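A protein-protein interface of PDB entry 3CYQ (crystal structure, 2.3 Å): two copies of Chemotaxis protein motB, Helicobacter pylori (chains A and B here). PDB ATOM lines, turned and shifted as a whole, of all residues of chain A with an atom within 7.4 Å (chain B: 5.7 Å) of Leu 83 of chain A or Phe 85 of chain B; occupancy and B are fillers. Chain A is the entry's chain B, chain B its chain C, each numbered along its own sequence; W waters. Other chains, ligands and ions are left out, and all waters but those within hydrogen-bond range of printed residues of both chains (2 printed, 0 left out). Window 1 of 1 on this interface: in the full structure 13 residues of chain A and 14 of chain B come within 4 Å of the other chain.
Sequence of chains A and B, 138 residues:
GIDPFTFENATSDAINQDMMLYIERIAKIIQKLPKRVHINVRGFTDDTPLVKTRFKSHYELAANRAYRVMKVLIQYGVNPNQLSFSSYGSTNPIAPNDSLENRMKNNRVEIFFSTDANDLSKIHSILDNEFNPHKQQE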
ATOM      1  N   ILE A  30     -35.872  22.237  19.916  1.00  0.00           N
ATOM      2  CA  ILE A  30     -35.139  22.729  18.771  1.00  0.00           C
ATOM      3  C   ILE A  30     -34.792  21.555  17.898  1.00  0.00           C
ATOM      4  O   ILE A  30     -34.873  21.675  16.693  1.00  0.00           O
ATOM      5  CB  ILE A  30     -33.831  23.508  19.168  1.00  0.00           C
ATOM      6  CG1 ILE A  30     -34.164  24.810  19.845  1.00  0.00           C
ATOM      7  CG2 ILE A  30     -32.975  23.914  17.957  1.00  0.00           C
ATOM      8  CD1 ILE A  30     -32.922  25.550  20.381  1.00  0.00           C
ATOM      9  N   VAL A  37     -34.931  25.848  10.170  1.00  0.00           N
ATOM     10  CA  VAL A  37     -35.239  26.765  11.244  1.00  0.00           C
ATOM     11  C   VAL A  37     -33.948  27.103  12.038  1.00  0.00           C
ATOM     12  O   VAL A  37     -33.193  26.237  12.427  1.00  0.00           O
ATOM     13  CB  VAL A  37     -36.415  26.234  12.132  1.00  0.00           C
ATOM     14  CG1 VAL A  37     -36.769  27.218  13.266  1.00  0.00           C
ATOM     15  CG2 VAL A  37     -37.660  25.999  11.280  1.00  0.00           C
ATOM     16  N   HIS A  38     -33.667  28.380  12.227  1.00  0.00           N
ATOM     17  CA  HIS A  38     -32.508  28.796  12.991  1.00  0.00           C
ATOM     18  C   HIS A  38     -32.981  29.487  14.255  1.00  0.00           C
ATOM     19  O   HIS A  38     -34.144  29.936  14.345  1.00  0.00           O
ATOM     20  CB  HIS A  38     -31.584  29.674  12.147  1.00  0.00           C
ATOM     21  CG  HIS A  38     -30.709  28.881  11.214  1.00  0.00           C
ATOM     22  ND1 HIS A  38     -29.386  29.189  10.987  1.00  0.00           N
ATOM     23  CD2 HIS A  38     -30.966  27.772  10.476  1.00  0.00           C
ATOM     24  CE1 HIS A  38     -28.869  28.316  10.139  1.00  0.00           C
ATOM     25  NE2 HIS A  38     -29.806  27.440   9.820  1.00  0.00           N
ATOM     26  N   ILE A  39     -32.073  29.514  15.230  1.00  0.00           N
ATOM     27  CA  ILE A  39     -32.341  29.961  16.597  1.00  0.00           C
ATOM     28  C   ILE A  39     -31.358  31.072  17.017  1.00  0.00           C
ATOM     29  O   ILE A  39     -30.160  30.915  16.961  1.00  0.00           O
ATOM     30  CB  ILE A  39     -32.297  28.769  17.585  1.00  0.00           C
ATOM     31  CG1 ILE A  39     -33.274  27.647  17.167  1.00  0.00           C
ATOM     32  CG2 ILE A  39     -32.579  29.241  19.006  1.00  0.00           C
ATOM     33  CD1 ILE A  39     -34.754  27.952  17.422  1.00  0.00           C
ATOM     34  N   ASN A  40     -31.896  32.209  17.442  1.00  0.00           N
ATOM     35  CA  ASN A  40     -31.122  33.346  17.915  1.00  0.00           C
ATOM     36  C   ASN A  40     -31.522  33.516  19.384  1.00  0.00           C
ATOM     37  O   ASN A  40     -32.687  33.743  19.712  1.00  0.00           O
ATOM     38  CB  ASN A  40     -31.406  34.607  17.088  1.00  0.00           C
ATOM     39  CG  ASN A  40     -30.627  35.840  17.570  1.00  0.00           C
ATOM     40  OD1 ASN A  40     -31.209  36.858  17.987  1.00  0.00           O
ATOM     41  ND2 ASN A  40     -29.311  35.768  17.470  1.00  0.00           N
ATOM     42  N   VAL A  41     -30.519  33.394  20.248  1.00  0.00           N
ATOM     43  CA  VAL A  41     -30.633  33.501  21.697  1.00  0.00           C
ATOM     44  C   VAL A  41     -30.312  34.953  22.048  1.00  0.00           C
ATOM     45  O   VAL A  41     -29.168  35.400  21.854  1.00  0.00           O
ATOM     46  CB  VAL A  41     -29.564  32.541  22.377  1.00  0.00           C
ATOM     47  CG1 VAL A  41     -29.607  32.588  23.909  1.00  0.00           C
ATOM     48  CG2 VAL A  41     -29.659  31.124  21.821  1.00  0.00           C
ATOM     49  N   TYR A  67     -24.701  34.095  25.345  1.00  0.00           N
ATOM     50  CA  TYR A  67     -23.678  33.153  24.996  1.00  0.00           C
ATOM     51  C   TYR A  67     -23.726  31.870  25.853  1.00  0.00           C
ATOM     52  O   TYR A  67     -23.590  30.756  25.367  1.00  0.00           O
ATOM     53  CB  TYR A  67     -22.331  33.854  25.173  1.00  0.00           C
ATOM     54  CG  TYR A  67     -21.172  32.914  25.063  1.00  0.00           C
ATOM     55  CD1 TYR A  67     -20.967  32.227  23.883  1.00  0.00           C
ATOM     56  CD2 TYR A  67     -20.294  32.682  26.140  1.00  0.00           C
ATOM     57  CE1 TYR A  67     -19.932  31.363  23.742  1.00  0.00           C
ATOM     58  CE2 TYR A  67     -19.245  31.792  25.997  1.00  0.00           C
ATOM     59  CZ  TYR A  67     -19.076  31.140  24.778  1.00  0.00           C
ATOM     60  OH  TYR A  67     -18.079  30.238  24.504  1.00  0.00           O
ATOM     61  N   VAL A  69     -26.375  30.563  27.586  1.00  0.00           N
ATOM     62  CA  VAL A  69     -27.565  29.762  27.293  1.00  0.00           C
ATOM     63  C   VAL A  69     -27.367  28.961  25.982  1.00  0.00           C
ATOM     64  O   VAL A  69     -27.743  27.789  25.880  1.00  0.00           O
ATOM     65  CB  VAL A  69     -28.865  30.621  27.244  1.00  0.00           C
ATOM     66  CG1 VAL A  69     -30.010  29.845  26.601  1.00  0.00           C
ATOM     67  CG2 VAL A  69     -29.277  31.092  28.661  1.00  0.00           C
ATOM     68  N   MET A  70     -26.772  29.607  24.981  1.00  0.00           N
ATOM     69  CA  MET A  70     -26.506  28.985  23.689  1.00  0.00           C
ATOM     70  C   MET A  70     -25.526  27.818  23.865  1.00  0.00           C
ATOM     71  O   MET A  70     -25.641  26.808  23.216  1.00  0.00           O
ATOM     72  CB  MET A  70     -25.956  30.037  22.724  1.00  0.00           C
ATOM     73  CG  MET A  70     -25.603  29.443  21.361  1.00  0.00           C
ATOM     74  SD  MET A  70     -24.815  30.524  20.196  1.00  0.00           S
ATOM     75  CE  MET A  70     -23.166  30.668  20.816  1.00  0.00           C
ATOM     76  N   LYS A  71     -24.574  27.976  24.771  1.00  0.00           N
ATOM     77  CA  LYS A  71     -23.613  26.947  25.087  1.00  0.00           C
ATOM     78  C   LYS A  71     -24.264  25.787  25.819  1.00  0.00           C
ATOM     79  O   LYS A  71     -23.918  24.619  25.603  1.00  0.00           O
ATOM     80  CB  LYS A  71     -22.469  27.624  25.846  1.00  0.00           C
ATOM     81  CG  LYS A  71     -21.312  26.803  26.278  1.00  0.00           C
ATOM     82  CD  LYS A  71     -20.038  27.650  26.373  1.00  0.00           C
ATOM     83  CE  LYS A  71     -19.944  28.506  27.595  1.00  0.00           C
ATOM     84  NZ  LYS A  71     -19.076  27.882  28.644  1.00  0.00           N
ATOM     85  N   VAL A  72     -25.249  26.060  26.667  1.00  0.00           N
ATOM     86  CA  VAL A  72     -25.978  24.936  27.261  1.00  0.00           C
ATOM     87  C   VAL A  72     -26.807  24.199  26.178  1.00  0.00           C
ATOM     88  O   VAL A  72     -26.864  22.977  26.162  1.00  0.00           O
ATOM     89  CB  VAL A  72     -26.798  25.329  28.507  1.00  0.00           C
ATOM     90  CG1 VAL A  72     -27.591  24.108  29.008  1.00  0.00           C
ATOM     91  CG2 VAL A  72     -25.890  25.888  29.618  1.00  0.00           C
ATOM     92  N   LEU A  73     -27.429  24.934  25.267  1.00  0.00           N
ATOM     93  CA  LEU A  73     -28.163  24.316  24.156  1.00  0.00           C
ATOM     94  C   LEU A  73     -27.247  23.384  23.333  1.00  0.00           C
ATOM     95  O   LEU A  73     -27.608  22.267  22.970  1.00  0.00           O
ATOM     96  CB  LEU A  73     -28.799  25.403  23.269  1.00  0.00           C
ATOM     97  CG  LEU A  73     -29.968  26.198  23.868  1.00  0.00           C
ATOM     98  CD1 LEU A  73     -30.302  27.468  23.039  1.00  0.00           C
ATOM     99  CD2 LEU A  73     -31.216  25.289  24.078  1.00  0.00           C
ATOM    100  N   ILE A  74     -26.037  23.852  23.041  1.00  0.00           N
ATOM    101  CA  ILE A  74     -25.074  23.060  22.297  1.00  0.00           C
ATOM    102  C   ILE A  74     -24.731  21.796  23.098  1.00  0.00           C
ATOM    103  O   ILE A  74     -24.594  20.720  22.547  1.00  0.00           O
ATOM    104  CB  ILE A  74     -23.841  23.920  21.961  1.00  0.00           C
ATOM    105  CG1 ILE A  74     -24.217  24.887  20.854  1.00  0.00           C
ATOM    106  CG2 ILE A  74     -22.655  23.083  21.511  1.00  0.00           C
ATOM    107  CD1 ILE A  74     -23.163  25.913  20.559  1.00  0.00           C
ATOM    108  N   GLN A  75     -24.644  21.922  24.410  1.00  0.00           N
ATOM    109  CA  GLN A  75     -24.337  20.789  25.274  1.00  0.00           C
ATOM    110  C   GLN A  75     -25.423  19.708  25.237  1.00  0.00           C
ATOM    111  O   GLN A  75     -25.132  18.512  25.388  1.00  0.00           O
ATOM    112  CB  GLN A  75     -24.201  21.318  26.691  1.00  0.00           C
ATOM    113  CG  GLN A  75     -23.401  20.489  27.611  1.00  0.00           C
ATOM    114  CD  GLN A  75     -23.544  20.999  29.034  1.00  0.00           C
ATOM    115  OE1 GLN A  75     -23.948  22.145  29.263  1.00  0.00           O
ATOM    116  NE2 GLN A  75     -23.225  20.144  30.003  1.00  0.00           N
ATOM    117  N   GLY A  77     -27.094  18.910  22.607  1.00  0.00           N
ATOM    118  CA  GLY A  77     -27.167  18.412  21.247  1.00  0.00           C
ATOM    119  C   GLY A  77     -27.595  19.375  20.143  1.00  0.00           C
ATOM    120  O   GLY A  77     -27.576  18.986  18.999  1.00  0.00           O
ATOM    121  N   VAL A  78     -27.971  20.615  20.434  1.00  0.00           N
ATOM    122  CA  VAL A  78     -28.354  21.495  19.342  1.00  0.00           C
ATOM    123  C   VAL A  78     -27.128  21.788  18.432  1.00  0.00           C
ATOM    124  O   VAL A  78     -26.001  22.006  18.909  1.00  0.00           O
ATOM    125  CB  VAL A  78     -29.029  22.803  19.834  1.00  0.00           C
ATOM    126  CG1 VAL A  78     -29.316  23.709  18.617  1.00  0.00           C
ATOM    127  CG2 VAL A  78     -30.311  22.501  20.630  1.00  0.00           C
ATOM    128  N   ASN A  79     -27.338  21.793  17.114  1.00  0.00           N
ATOM    129  CA  ASN A  79     -26.216  22.049  16.217  1.00  0.00           C
ATOM    130  C   ASN A  79     -25.785  23.505  16.233  1.00  0.00           C
ATOM    131  O   ASN A  79     -26.617  24.353  16.110  1.00  0.00           O
ATOM    132  CB  ASN A  79     -26.479  21.595  14.776  1.00  0.00           C
ATOM    133  CG  ASN A  79     -25.162  21.329  14.015  1.00  0.00           C
ATOM    134  OD1 ASN A  79     -24.515  22.252  13.495  1.00  0.00           O
ATOM    135  ND2 ASN A  79     -24.747  20.051  13.988  1.00  0.00           N
ATOM    136  N   PRO A  80     -24.480  23.798  16.393  1.00  0.00           N
ATOM    137  CA  PRO A  80     -24.022  25.173  16.248  1.00  0.00           C
ATOM    138  C   PRO A  80     -24.505  25.866  14.972  1.00  0.00           C
ATOM    139  O   PRO A  80     -24.723  27.064  14.989  1.00  0.00           O
ATOM    140  CB  PRO A  80     -22.507  25.017  16.264  1.00  0.00           C
ATOM    141  CG  PRO A  80     -22.270  23.920  17.169  1.00  0.00           C
ATOM    142  CD  PRO A  80     -23.344  22.928  16.763  1.00  0.00           C
ATOM    143  N   ASN A  81     -24.700  25.123  13.892  1.00  0.00           N
ATOM    144  CA  ASN A  81     -25.093  25.720  12.627  1.00  0.00           C
ATOM    145  C   ASN A  81     -26.447  26.433  12.707  1.00  0.00           C
ATOM    146  O   ASN A  81     -26.643  27.483  12.076  1.00  0.00           O
ATOM    147  CB  ASN A  81     -25.044  24.693  11.491  1.00  0.00           C
ATOM    148  CG  ASN A  81     -25.066  25.373  10.136  1.00  0.00           C
ATOM    149  OD1 ASN A  81     -24.287  26.306   9.871  1.00  0.00           O
ATOM    150  ND2 ASN A  81     -25.970  24.932   9.285  1.00  0.00           N
ATOM    151  N   GLN A  82     -27.342  25.921  13.554  1.00  0.00           N
ATOM    152  CA  GLN A  82     -28.638  26.561  13.774  1.00  0.00           C
ATOM    153  C   GLN A  82     -28.689  27.730  14.768  1.00  0.00           C
ATOM    154  O   GLN A  82     -29.781  28.263  15.031  1.00  0.00           O
ATOM    155  CB  GLN A  82     -29.636  25.499  14.221  1.00  0.00           C
ATOM    156  CG  GLN A  82     -29.864  24.469  13.153  1.00  0.00           C
ATOM    157  CD  GLN A  82     -30.700  23.363  13.679  1.00  0.00           C
ATOM    158  OE1 GLN A  82     -30.162  22.408  14.231  1.00  0.00           O
ATOM    159  NE2 GLN A  82     -32.031  23.487  13.544  1.00  0.00           N
ATOM    160  N   LEU A  83     -27.544  28.123  15.320  1.00  0.00           N
ATOM    161  CA  LEU A  83     -27.517  28.986  16.512  1.00  0.00           C
ATOM    162  C   LEU A  83     -26.654  30.214  16.381  1.00  0.00           C
ATOM    163  O   LEU A  83     -25.643  30.198  15.679  1.00  0.00           O
ATOM    164  CB  LEU A  83     -27.039  28.216  17.747  1.00  0.00           C
ATOM    165  CG  LEU A  83     -27.990  27.196  18.411  1.00  0.00           C
ATOM    166  CD1 LEU A  83     -27.152  26.311  19.343  1.00  0.00           C
ATOM    167  CD2 LEU A  83     -29.193  27.851  19.136  1.00  0.00           C
ATOM    168  N   SER A  84     -27.086  31.260  17.083  1.00  0.00           N
ATOM    169  CA  SER A  84     -26.382  32.537  17.240  1.00  0.00           C
ATOM    170  C   SER A  84     -26.844  33.136  18.562  1.00  0.00           C
ATOM    171  O   SER A  84     -27.818  32.689  19.149  1.00  0.00           O
ATOM    172  CB  SER A  84     -26.652  33.524  16.073  1.00  0.00           C
ATOM    173  OG  SER A  84     -28.027  33.606  15.689  1.00  0.00           O
ATOM    174  N   PHE A  85     -26.129  34.152  19.026  1.00  0.00           N
ATOM    175  CA  PHE A  85     -26.524  34.885  20.211  1.00  0.00           C
ATOM    176  C   PHE A  85     -26.457  36.392  19.947  1.00  0.00           C
ATOM    177  O   PHE A  85     -25.707  36.827  19.115  1.00  0.00           O
ATOM    178  CB  PHE A  85     -25.661  34.475  21.409  1.00  0.00           C
ATOM    179  CG  PHE A  85     -24.239  34.959  21.359  1.00  0.00           C
ATOM    180  CD1 PHE A  85     -23.285  34.252  20.663  1.00  0.00           C
ATOM    181  CD2 PHE A  85     -23.859  36.100  22.030  1.00  0.00           C
ATOM    182  CE1 PHE A  85     -21.986  34.691  20.628  1.00  0.00           C
ATOM    183  CE2 PHE A  85     -22.578  36.523  22.009  1.00  0.00           C
ATOM    184  CZ  PHE A  85     -21.638  35.838  21.306  1.00  0.00           C
ATOM    185  N   ILE A 111     -35.690  33.461  23.105  1.00  0.00           N
ATOM    186  CA  ILE A 111     -35.402  32.624  21.965  1.00  0.00           C
ATOM    187  C   ILE A 111     -36.213  33.146  20.776  1.00  0.00           C
ATOM    188  O   ILE A 111     -37.438  33.197  20.871  1.00  0.00           O
ATOM    189  CB  ILE A 111     -35.722  31.133  22.247  1.00  0.00           C
ATOM    190  CG1 ILE A 111     -34.925  30.613  23.476  1.00  0.00           C
ATOM    191  CG2 ILE A 111     -35.475  30.268  20.996  1.00  0.00           C
ATOM    192  CD1 ILE A 111     -33.391  30.595  23.335  1.00  0.00           C
ATOM    193  N   ILE B  39     -16.049  41.287  15.833  1.00  0.00           N
ATOM    194  CA  ILE B  39     -15.282  40.228  15.243  1.00  0.00           C
ATOM    195  C   ILE B  39     -16.218  39.073  14.911  1.00  0.00           C
ATOM    196  O   ILE B  39     -16.877  38.555  15.771  1.00  0.00           O
ATOM    197  CB  ILE B  39     -14.195  39.745  16.184  1.00  0.00           C
ATOM    198  CG1 ILE B  39     -13.233  40.886  16.571  1.00  0.00           C
ATOM    199  CG2 ILE B  39     -13.447  38.545  15.539  1.00  0.00           C
ATOM    200  CD1 ILE B  39     -12.148  41.127  15.575  1.00  0.00           C
ATOM    201  N   ASN B  40     -16.225  38.687  13.645  1.00  0.00           N
ATOM    202  CA  ASN B  40     -16.948  37.571  13.131  1.00  0.00           C
ATOM    203  C   ASN B  40     -15.954  36.434  12.852  1.00  0.00           C
ATOM    204  O   ASN B  40     -15.013  36.598  12.086  1.00  0.00           O
ATOM    205  CB  ASN B  40     -17.647  38.007  11.858  1.00  0.00           C
ATOM    206  CG  ASN B  40     -18.524  36.939  11.271  1.00  0.00           C
ATOM    207  OD1 ASN B  40     -18.339  36.552  10.118  1.00  0.00           O
ATOM    208  ND2 ASN B  40     -19.480  36.448  12.058  1.00  0.00           N
ATOM    209  N   VAL B  41     -16.174  35.291  13.505  1.00  0.00           N
ATOM    210  CA  VAL B  41     -15.340  34.106  13.337  1.00  0.00           C
ATOM    211  C   VAL B  41     -16.014  33.188  12.296  1.00  0.00           C
ATOM    212  O   VAL B  41     -17.135  32.746  12.504  1.00  0.00           O
ATOM    213  CB  VAL B  41     -15.156  33.386  14.701  1.00  0.00           C
ATOM    214  CG1 VAL B  41     -14.052  32.342  14.609  1.00  0.00           C
ATOM    215  CG2 VAL B  41     -14.865  34.411  15.764  1.00  0.00           C
ATOM    216  N   ARG B  42     -15.346  32.936  11.173  1.00  0.00           N
ATOM    217  CA  ARG B  42     -15.949  32.251  10.031  1.00  0.00           C
ATOM    218  C   ARG B  42     -15.268  30.911   9.768  1.00  0.00           C
ATOM    219  O   ARG B  42     -14.034  30.867   9.655  1.00  0.00           O
ATOM    220  CB  ARG B  42     -15.810  33.070   8.751  1.00  0.00           C
ATOM    221  CG  ARG B  42     -16.345  34.444   8.842  1.00  0.00           C
ATOM    222  CD  ARG B  42     -16.450  35.099   7.477  1.00  0.00           C
ATOM    223  NE  ARG B  42     -17.170  36.359   7.646  1.00  0.00           N
ATOM    224  CZ  ARG B  42     -17.497  37.209   6.679  1.00  0.00           C
ATOM    225  NH1 ARG B  42     -17.207  36.967   5.407  1.00  0.00           N
ATOM    226  NH2 ARG B  42     -18.143  38.316   7.012  1.00  0.00           N
ATOM    227  N   ALA B  63     -19.337  25.217  11.018  1.00  0.00           N
ATOM    228  CA  ALA B  63     -19.994  25.808  12.161  1.00  0.00           C
ATOM    229  C   ALA B  63     -19.380  25.332  13.474  1.00  0.00           C
ATOM    230  O   ALA B  63     -19.148  26.120  14.400  1.00  0.00           O
ATOM    231  CB  ALA B  63     -21.546  25.522  12.110  1.00  0.00           C
ATOM    232  N   ALA B  66     -15.830  27.152  13.652  1.00  0.00           N
ATOM    233  CA  ALA B  66     -15.999  28.567  13.950  1.00  0.00           C
ATOM    234  C   ALA B  66     -16.421  28.774  15.408  1.00  0.00           C
ATOM    235  O   ALA B  66     -15.850  29.593  16.137  1.00  0.00           O
ATOM    236  CB  ALA B  66     -17.035  29.199  12.953  1.00  0.00           C
ATOM    237  N   TYR B  67     -17.416  28.009  15.836  1.00  0.00           N
ATOM    238  CA  TYR B  67     -17.901  28.107  17.201  1.00  0.00           C
ATOM    239  C   TYR B  67     -16.773  27.803  18.221  1.00  0.00           C
ATOM    240  O   TYR B  67     -16.615  28.485  19.230  1.00  0.00           O
ATOM    241  CB  TYR B  67     -19.076  27.151  17.366  1.00  0.00           C
ATOM    242  CG  TYR B  67     -19.404  26.895  18.805  1.00  0.00           C
ATOM    243  CD1 TYR B  67     -20.009  27.886  19.556  1.00  0.00           C
ATOM    244  CD2 TYR B  67     -19.097  25.678  19.419  1.00  0.00           C
ATOM    245  CE1 TYR B  67     -20.319  27.697  20.887  1.00  0.00           C
ATOM    246  CE2 TYR B  67     -19.398  25.469  20.766  1.00  0.00           C
ATOM    247  CZ  TYR B  67     -20.019  26.492  21.493  1.00  0.00           C
ATOM    248  OH  TYR B  67     -20.374  26.373  22.818  1.00  0.00           O
ATOM    249  N   MET B  70     -14.202  30.594  18.379  1.00  0.00           N
ATOM    250  CA  MET B  70     -14.899  31.670  19.123  1.00  0.00           C
ATOM    251  C   MET B  70     -14.945  31.436  20.655  1.00  0.00           C
ATOM    252  O   MET B  70     -14.685  32.349  21.426  1.00  0.00           O
ATOM    253  CB  MET B  70     -16.314  31.859  18.567  1.00  0.00           C
ATOM    254  CG  MET B  70     -16.961  33.144  19.022  1.00  0.00           C
ATOM    255  SD  MET B  70     -18.738  33.243  18.829  1.00  0.00           S
ATOM    256  CE  MET B  70     -19.296  31.803  19.742  1.00  0.00           C
ATOM    257  N   LEU B  83     -18.191  39.331  19.696  1.00  0.00           N
ATOM    258  CA  LEU B  83     -18.006  38.133  18.894  1.00  0.00           C
ATOM    259  C   LEU B  83     -19.282  37.549  18.286  1.00  0.00           C
ATOM    260  O   LEU B  83     -20.349  37.663  18.883  1.00  0.00           O
ATOM    261  CB  LEU B  83     -17.326  37.041  19.740  1.00  0.00           C
ATOM    262  CG  LEU B  83     -15.852  37.172  20.107  1.00  0.00           C
ATOM    263  CD1 LEU B  83     -15.540  36.249  21.246  1.00  0.00           C
ATOM    264  CD2 LEU B  83     -15.054  36.887  18.833  1.00  0.00           C
ATOM    265  N   SER B  84     -19.134  36.939  17.098  1.00  0.00           N
ATOM    266  CA  SER B  84     -20.145  36.107  16.420  1.00  0.00           C
ATOM    267  C   SER B  84     -19.417  35.032  15.613  1.00  0.00           C
ATOM    268  O   SER B  84     -18.196  35.129  15.417  1.00  0.00           O
ATOM    269  CB  SER B  84     -21.068  36.902  15.497  1.00  0.00           C
ATOM    270  OG  SER B  84     -20.311  37.732  14.656  1.00  0.00           O
ATOM    271  N   PHE B  85     -20.137  34.005  15.176  1.00  0.00           N
ATOM    272  CA  PHE B  85     -19.520  32.932  14.370  1.00  0.00           C
ATOM    273  C   PHE B  85     -20.451  32.689  13.223  1.00  0.00           C
ATOM    274  O   PHE B  85     -21.649  32.863  13.373  1.00  0.00           O
ATOM    275  CB  PHE B  85     -19.227  31.619  15.125  1.00  0.00           C
ATOM    276  CG  PHE B  85     -20.467  30.751  15.458  1.00  0.00           C
ATOM    277  CD1 PHE B  85     -21.252  31.011  16.591  1.00  0.00           C
ATOM    278  CD2 PHE B  85     -20.820  29.651  14.663  1.00  0.00           C
ATOM    279  CE1 PHE B  85     -22.372  30.234  16.914  1.00  0.00           C
ATOM    280  CE2 PHE B  85     -21.954  28.858  14.988  1.00  0.00           C
ATOM    281  CZ  PHE B  85     -22.715  29.156  16.130  1.00  0.00           C
ATOM    282  N   SER B  86     -19.877  32.271  12.098  1.00  0.00           N
ATOM    283  CA  SER B  86     -20.604  32.013  10.867  1.00  0.00           C
ATOM    284  C   SER B  86     -20.037  30.827  10.103  1.00  0.00           C
ATOM    285  O   SER B  86     -18.817  30.674  10.025  1.00  0.00           O
ATOM    286  CB  SER B  86     -20.502  33.279  10.014  1.00  0.00           C
ATOM    287  OG  SER B  86     -21.040  34.364  10.736  1.00  0.00           O
ATOM    288  N   SER B  87     -20.906  29.989   9.553  1.00  0.00           N
ATOM    289  CA  SER B  87     -20.498  28.857   8.715  1.00  0.00           C
ATOM    290  C   SER B  87     -20.762  29.139   7.243  1.00  0.00           C
ATOM    291  O   SER B  87     -21.868  29.556   6.860  1.00  0.00           O
ATOM    292  CB  SER B  87     -21.228  27.546   9.050  1.00  0.00           C
ATOM    293  OG  SER B  87     -20.738  26.475   8.231  1.00  0.00           O
HETATM  294  O   HOH W   1     -24.191  31.719  13.924  1.00  0.00           O
HETATM  295  O   HOH W   2     -21.146  23.649  24.360  1.00  0.00           O
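Among the printed residues, merely in contact across the chains: Lys 71 of chain A with Tyr 67 of chain B (3.6 Å), Ile 74 of chain A with Tyr 67 of chain B (3.3 Å), Pro 80 of chain A with Ala 63 of chain B (3.997 Å), Pro 80 of chain A with Phe 85 of chain B (3.1 Å), Asn 81 of chain A with Ala 63 of chain B (3.6 Å), Asn 81 of chain A with Ser 87 of chain B (3.4 Å), Leu 83 of chain A with Phe 85 of chain B (3.1 Å), Phe 85 of chain A with Met 70 of chain B (3.99 Å) and Phe 85 of chain A with Leu 83 of chain B (3.3 Å).
Leu 83 of chain A touches Phe 85 of chain B, and with the chains exchanged Phe 85 of chain A touches Leu 83 of chain B. Phe 85 of chain A touches Met 70 of chain B, but with the chains exchanged Met 70 of chain A does not touch Phe 85 of chain B (4.01 Å). Positions printed for both chains: 39, 40, 41, 67, 70, 83, 84 and 85. Of the 9 pairs that touch across the chains among the printed residues, 2 have their exchanged pair printed and touching as well.
Leu 83 of chain A touches one residue of chain B. Printed residues of chain A within 4 Å of Phe 85 of chain B: Pro 80 and Leu 83. Of the printed residues of chain B, Ile 74 of chain A touches Tyr 67. Printed residues of chain B within 4 Å of Asn 81 of chain A: Ala 63 (3.6 Å) and Ser 87 (3.4 Å). Of the printed residues of chain A, Ser 87 of chain B touches Asn 81. Of the printed residues of chain A, Ala 63 of chain B touches Pro 80 (3.997 Å) and Asn 81 (3.6 Å). Leu 73 of chain A touches none of the printed residues of chain B. Val 78 of chain A touches none of the printed residues of chain B.
Water W1 bridges O of Leu 83 of chain A and O of Phe 85 of chain B. Water W2 lies within hydrogen-bond range of O of Lys 71 of chain A (3.2 Å) and OH of Tyr 67 of chain B (3.2 Å).
Of the 24 printed residues of chain A, 6 touch a printed residue of chain B. Among the printed residues, 9 pairs touch across the chains. Among the printed residues, no Asp or Glu carboxylate lies within 4 Å of a Lys or Arg side-chain nitrogen of the other chain.
A ring nitrogen (ND1) of His 38 of chain A sits close to the backbone carbonyl oxygen (O) of Asn 81 of chain A (3.4 Å). OD1 of Asn 79 of chain A is in hydrogen-bond range of N of Asn 81 of chain A (2.9 Å). N of Ala 63 of chain B lies within hydrogen-bond range of OG of Ser 87 of chain B, at 3.4 Å.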
